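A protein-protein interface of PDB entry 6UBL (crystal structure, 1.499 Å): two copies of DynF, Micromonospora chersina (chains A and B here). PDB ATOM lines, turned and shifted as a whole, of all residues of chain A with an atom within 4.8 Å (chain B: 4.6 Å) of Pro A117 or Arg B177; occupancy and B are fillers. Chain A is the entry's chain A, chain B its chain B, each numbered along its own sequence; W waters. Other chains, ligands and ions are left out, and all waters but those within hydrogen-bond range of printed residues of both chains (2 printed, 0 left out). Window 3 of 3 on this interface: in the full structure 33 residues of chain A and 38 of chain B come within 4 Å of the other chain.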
ATOM      1  N   ARG A 115     -25.137   3.153 -15.626  1.00  0.00           N
ATOM      2  CA  ARG A 115     -24.125   2.123 -15.468  1.00  0.00           C
ATOM      3  C   ARG A 115     -22.758   2.751 -15.241  1.00  0.00           C
ATOM      4  O   ARG A 115     -22.535   3.929 -15.521  1.00  0.00           O
ATOM      5  CB  ARG A 115     -24.094   1.155 -16.659  1.00  0.00           C
ATOM      6  CG  ARG A 115     -23.703   1.762 -18.030  1.00  0.00           C
ATOM      7  CD  ARG A 115     -23.058   0.675 -18.894  1.00  0.00           C
ATOM      8  NE  ARG A 115     -21.774   0.338 -18.291  1.00  0.00           N
ATOM      9  CZ  ARG A 115     -21.260  -0.884 -18.159  1.00  0.00           C
ATOM     10  NH1 ARG A 115     -21.906  -1.953 -18.604  1.00  0.00           N
ATOM     11  NH2 ARG A 115     -20.082  -1.035 -17.562  1.00  0.00           N
ATOM     12  N   THR A 116     -21.842   1.933 -14.738  1.00  0.00           N
ATOM     13  CA  THR A 116     -20.450   2.356 -14.586  1.00  0.00           C
ATOM     14  C   THR A 116     -19.888   2.799 -15.934  1.00  0.00           C
ATOM     15  O   THR A 116     -20.021   2.069 -16.932  1.00  0.00           O
ATOM     16  CB  THR A 116     -19.633   1.184 -14.047  1.00  0.00           C
ATOM     17  OG1 THR A 116     -20.112   0.813 -12.745  1.00  0.00           O
ATOM     18  CG2 THR A 116     -18.146   1.514 -14.009  1.00  0.00           C
ATOM     19  N   PRO A 117     -19.275   3.978 -16.015  1.00  0.00           N
ATOM     20  CA  PRO A 117     -18.656   4.406 -17.273  1.00  0.00           C
ATOM     21  C   PRO A 117     -17.351   3.668 -17.547  1.00  0.00           C
ATOM     22  O   PRO A 117     -16.701   3.137 -16.646  1.00  0.00           O
ATOM     23  CB  PRO A 117     -18.415   5.906 -17.053  1.00  0.00           C
ATOM     24  CG  PRO A 117     -18.197   6.007 -15.555  1.00  0.00           C
ATOM     25  CD  PRO A 117     -19.145   4.999 -14.958  1.00  0.00           C
ATOM     26  N   PHE A 118     -16.964   3.656 -18.829  1.00  0.00           N
ATOM     27  CA  PHE A 118     -15.694   3.082 -19.269  1.00  0.00           C
ATOM     28  C   PHE A 118     -14.539   4.056 -19.098  1.00  0.00           C
ATOM     29  O   PHE A 118     -13.380   3.650 -19.219  1.00  0.00           O
ATOM     30  CB  PHE A 118     -15.848   2.569 -20.703  1.00  0.00           C
ATOM     31  CG  PHE A 118     -16.996   1.601 -20.846  1.00  0.00           C
ATOM     32  CD1 PHE A 118     -16.888   0.321 -20.323  1.00  0.00           C
ATOM     33  CD2 PHE A 118     -18.167   1.993 -21.432  1.00  0.00           C
ATOM     34  CE1 PHE A 118     -17.963  -0.560 -20.424  1.00  0.00           C
ATOM     35  CE2 PHE A 118     -19.244   1.119 -21.542  1.00  0.00           C
ATOM     36  CZ  PHE A 118     -19.123  -0.155 -21.034  1.00  0.00           C
ATOM     37  N   ASP A 119     -14.835   5.326 -18.807  1.00  0.00           N
ATOM     38  CA  ASP A 119     -13.843   6.388 -18.671  1.00  0.00           C
ATOM     39  C   ASP A 119     -14.026   7.058 -17.311  1.00  0.00           C
ATOM     40  O   ASP A 119     -14.490   8.203 -17.232  1.00  0.00           O
ATOM     41  CB  ASP A 119     -13.983   7.410 -19.801  1.00  0.00           C
ATOM     42  CG  ASP A 119     -15.312   8.151 -19.788  1.00  0.00           C
ATOM     43  OD1 ASP A 119     -16.389   7.522 -19.598  1.00  0.00           O
ATOM     44  OD2 ASP A 119     -15.285   9.386 -19.961  1.00  0.00           O
ATOM     45  N   PRO A 120     -13.752   6.328 -16.207  1.00  0.00           N
ATOM     46  CA  PRO A 120     -13.855   6.901 -14.852  1.00  0.00           C
ATOM     47  C   PRO A 120     -12.704   7.852 -14.510  1.00  0.00           C
ATOM     48  O   PRO A 120     -12.039   7.713 -13.482  1.00  0.00           O
ATOM     49  CB  PRO A 120     -13.824   5.658 -13.956  1.00  0.00           C
ATOM     50  CG  PRO A 120     -13.013   4.667 -14.728  1.00  0.00           C
ATOM     51  CD  PRO A 120     -13.371   4.904 -16.176  1.00  0.00           C
ATOM     52  N   ALA A 122     -12.849  11.406 -14.643  1.00  0.00           N
ATOM     53  CA  ALA A 122     -13.480  12.709 -14.651  1.00  0.00           C
ATOM     54  C   ALA A 122     -13.577  13.349 -13.276  1.00  0.00           C
ATOM     55  O   ALA A 122     -14.238  14.378 -13.141  1.00  0.00           O
ATOM     56  CB  ALA A 122     -14.880  12.589 -15.256  1.00  0.00           C
ATOM     57  N   GLU A 124     -15.167  12.037 -10.730  1.00  0.00           N
ATOM     58  CA  GLU A 124     -16.394  11.611 -10.103  1.00  0.00           C
ATOM     59  C   GLU A 124     -16.047  10.838  -8.846  1.00  0.00           C
ATOM     60  O   GLU A 124     -14.900  10.425  -8.641  1.00  0.00           O
ATOM     61  CB  GLU A 124     -17.095  10.664 -11.071  1.00  0.00           C
ATOM     62  CG  GLU A 124     -17.644  11.356 -12.308  1.00  0.00           C
ATOM     63  CD  GLU A 124     -18.025  10.375 -13.392  1.00  0.00           C
ATOM     64  OE1 GLU A 124     -17.176   9.516 -13.741  1.00  0.00           O
ATOM     65  OE2 GLU A 124     -19.166  10.440 -13.888  1.00  0.00           O
ATOM     66  N   ALA A 128     -18.954   6.029  -8.786  1.00  0.00           N
ATOM     67  CA  ALA A 128     -20.114   6.727  -9.325  1.00  0.00           C
ATOM     68  C   ALA A 128     -20.441   6.204 -10.721  1.00  0.00           C
ATOM     69  O   ALA A 128     -19.580   5.728 -11.459  1.00  0.00           O
ATOM     70  CB  ALA A 128     -19.847   8.232  -9.405  1.00  0.00           C
ATOM     71  N   LYS A 129     -21.698   6.340 -11.094  1.00  0.00           N
ATOM     72  CA  LYS A 129     -22.167   5.840 -12.372  1.00  0.00           C
ATOM     73  C   LYS A 129     -22.475   6.983 -13.325  1.00  0.00           C
ATOM     74  O   LYS A 129     -22.376   8.170 -12.981  1.00  0.00           O
ATOM     75  CB  LYS A 129     -23.359   4.902 -12.166  1.00  0.00           C
ATOM     76  CG  LYS A 129     -22.930   3.664 -11.388  1.00  0.00           C
ATOM     77  CD  LYS A 129     -24.021   2.613 -11.311  1.00  0.00           C
ATOM     78  CE  LYS A 129     -23.633   1.451 -10.391  1.00  0.00           C
ATOM     79  NZ  LYS A 129     -22.518   0.601 -10.910  1.00  0.00           N
ATOM     80  N   ALA A 130     -22.783   6.601 -14.562  1.00  0.00           N
ATOM     81  CA  ALA A 130     -23.123   7.543 -15.614  1.00  0.00           C
ATOM     82  C   ALA A 130     -24.534   7.235 -16.077  1.00  0.00           C
ATOM     83  O   ALA A 130     -24.881   6.078 -16.318  1.00  0.00           O
ATOM     84  CB  ALA A 130     -22.152   7.407 -16.779  1.00  0.00           C
ATOM     85  N   ASP A 159     -23.616  12.893 -14.978  1.00  0.00           N
ATOM     86  CA  ASP A 159     -22.395  12.236 -14.543  1.00  0.00           C
ATOM     87  C   ASP A 159     -22.344  12.242 -13.021  1.00  0.00           C
ATOM     88  O   ASP A 159     -23.166  12.873 -12.346  1.00  0.00           O
ATOM     89  CB  ASP A 159     -21.183  12.939 -15.154  1.00  0.00           C
ATOM     90  CG  ASP A 159     -21.199  12.893 -16.688  1.00  0.00           C
ATOM     91  OD1 ASP A 159     -21.473  11.820 -17.251  1.00  0.00           O
ATOM     92  OD2 ASP A 159     -20.953  13.938 -17.321  1.00  0.00           O
ATOM     93  N   ILE B 175     -19.845  11.157 -29.556  1.00  0.00           N
ATOM     94  CA  ILE B 175     -20.335  10.094 -28.689  1.00  0.00           C
ATOM     95  C   ILE B 175     -19.925  10.449 -27.276  1.00  0.00           C
ATOM     96  O   ILE B 175     -18.733  10.553 -26.974  1.00  0.00           O
ATOM     97  CB  ILE B 175     -19.754   8.731 -29.082  1.00  0.00           C
ATOM     98  CG1 ILE B 175     -20.233   8.349 -30.487  1.00  0.00           C
ATOM     99  CG2 ILE B 175     -20.150   7.687 -28.035  1.00  0.00           C
ATOM    100  CD1 ILE B 175     -19.358   7.317 -31.150  1.00  0.00           C
ATOM    101  N   TYR B 176     -20.906  10.628 -26.410  1.00  0.00           N
ATOM    102  CA  TYR B 176     -20.648  11.015 -25.030  1.00  0.00           C
ATOM    103  C   TYR B 176     -20.556   9.760 -24.169  1.00  0.00           C
ATOM    104  O   TYR B 176     -21.583   9.173 -23.772  1.00  0.00           O
ATOM    105  CB  TYR B 176     -21.747  11.916 -24.501  1.00  0.00           C
ATOM    106  CG  TYR B 176     -21.369  12.590 -23.216  1.00  0.00           C
ATOM    107  CD1 TYR B 176     -21.774  12.084 -21.990  1.00  0.00           C
ATOM    108  CD2 TYR B 176     -20.564  13.722 -23.222  1.00  0.00           C
ATOM    109  CE1 TYR B 176     -21.418  12.710 -20.815  1.00  0.00           C
ATOM    110  CE2 TYR B 176     -20.221  14.361 -22.060  1.00  0.00           C
ATOM    111  CZ  TYR B 176     -20.641  13.846 -20.847  1.00  0.00           C
ATOM    112  OH  TYR B 176     -20.274  14.483 -19.690  1.00  0.00           O
ATOM    113  N   ARG B 177     -19.309   9.358 -23.884  1.00  0.00           N
ATOM    114  CA  ARG B 177     -18.973   8.260 -22.977  1.00  0.00           C
ATOM    115  C   ARG B 177     -19.282   6.880 -23.550  1.00  0.00           C
ATOM    116  O   ARG B 177     -18.434   5.979 -23.469  1.00  0.00           O
ATOM    117  CB  ARG B 177     -19.564   8.427 -21.582  1.00  0.00           C
ATOM    118  CG  ARG B 177     -19.236   9.754 -20.934  1.00  0.00           C
ATOM    119  CD  ARG B 177     -19.549   9.766 -19.445  1.00  0.00           C
ATOM    120  NE  ARG B 177     -18.414   9.365 -18.624  1.00  0.00           N
ATOM    121  CZ  ARG B 177     -18.361   9.457 -17.306  1.00  0.00           C
ATOM    122  NH1 ARG B 177     -19.419   9.897 -16.629  1.00  0.00           N
ATOM    123  NH2 ARG B 177     -17.273   9.082 -16.656  1.00  0.00           N
ATOM    124  N   MET B 178     -20.486   6.685 -24.093  1.00  0.00           N
ATOM    125  CA  MET B 178     -20.852   5.366 -24.589  1.00  0.00           C
ATOM    126  C   MET B 178     -22.075   5.431 -25.490  1.00  0.00           C
ATOM    127  O   MET B 178     -23.042   6.139 -25.192  1.00  0.00           O
ATOM    128  CB  MET B 178     -21.125   4.420 -23.407  1.00  0.00           C
ATOM    129  CG  MET B 178     -22.389   4.768 -22.615  1.00  0.00           C
ATOM    130  SD  MET B 178     -22.594   3.837 -21.089  1.00  0.00           S
ATOM    131  CE  MET B 178     -21.404   4.589 -19.988  1.00  0.00           C
ATOM    132  N   THR B 196     -17.351   3.653 -27.892  1.00  0.00           N
ATOM    133  CA  THR B 196     -16.938   4.671 -26.937  1.00  0.00           C
ATOM    134  C   THR B 196     -16.221   5.851 -27.578  1.00  0.00           C
ATOM    135  O   THR B 196     -16.184   6.933 -26.976  1.00  0.00           O
ATOM    136  CB  THR B 196     -16.102   4.069 -25.807  1.00  0.00           C
ATOM    137  OG1 THR B 196     -14.953   3.390 -26.347  1.00  0.00           O
ATOM    138  CG2 THR B 196     -16.928   3.102 -24.969  1.00  0.00           C
HETATM  139  O   HOH W   1     -17.734   5.537 -20.812  1.00  0.00           O
HETATM  140  O   HOH W   2     -24.824   5.739 -19.239  1.00  0.00           O
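The guanidinium group of Arg B177 is in salt-bridge range of the side-chain carboxylate of Asp A119 (2.9 Å).
The side-chain carboxylate (OE2) of Glu A124 is in salt-bridge range of the guanidinium group (NH1) of Arg B177 (2.8 Å).
The side-chain carboxylate of Asp A159 is in hydrogen-bond range of the side-chain hydroxyl of Tyr B176 (2.5 Å).
The side-chain carboxylate (OD1) of Asp A159 lies within salt-bridge range of the guanidinium group (NH1) of Arg B177.
The backbone NH (N) of Ala A130 lies within hydrogen-bond range of the backbone carbonyl oxygen (O) of Arg A115, 2.8 Å away.
Among the printed residues, merely in contact across the chains: Pro A117 with Arg B177, Ala A130 with Arg B177, Arg A115 with Met B178, Pro A117 with Met B178 and Phe A118 with Thr B196.
Of the printed residues of chain B, Arg A115 touches Met B178.
Of chain B, only Arg B177 and Met B178 come within 4 Å of Pro A117.
Of the printed residues of chain B, Asp A119 touches Arg B177.
Ala A122 touches none of the printed residues of chain B.
Ala A128 touches none of the printed residues of chain B.
Of chain A, only Pro A117, Asp A119, Glu A124, Ala A130 and Asp A159 come within 4 Å of Arg B177.
Of the printed residues of chain A, Met B178 touches Arg A115 and Pro A117.
The nearest printed residue of chain B that does not touch Pro A117 is Thr B196 (7.5 Å).
Of the 5 printed residues of chain B, 4 touch a printed residue of chain A.
Printed residues of chain B that touch a printed residue of chain A: Tyr B176, Arg B177, Met B178 and Thr B196.
Hydrophobic or aromatic side chains of chain B within 4 Å of the printed part of chain A: Tyr B176 and Met B178.
Of the 12 printed residues of chain A, 7 touch a printed residue of chain B.
Hydrophobic or aromatic side chains of chain A within 4 Å of the printed part of chain B: Pro A117, Phe A118 and Ala A130.
Among the printed residues, Asp or Glu carboxylates within 4 Å of a Lys or Arg side-chain nitrogen of the other chain: Asp A119 with Arg B177 (2.9 Å), Glu A124 with Arg B177 (2.8 Å) and Asp A159 with Arg B177 (2.9 Å).
No position is printed for both chains.
Of the 9 pairs that touch across the chains among the printed residues, none has its exchanged pair printed and touching as well.
Water W1 lies within hydrogen-bond range of the side-chain carboxylate (OD1) of Asp A119, the backbone carbonyl oxygen (O) of Arg B177 and the backbone NH (N) of Phe A118.
Water W2 bridges the backbone carbonyl oxygen of Ala A130 (2.9 Å) and the side-chain sulfur of Met B178 (3.5 Å).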
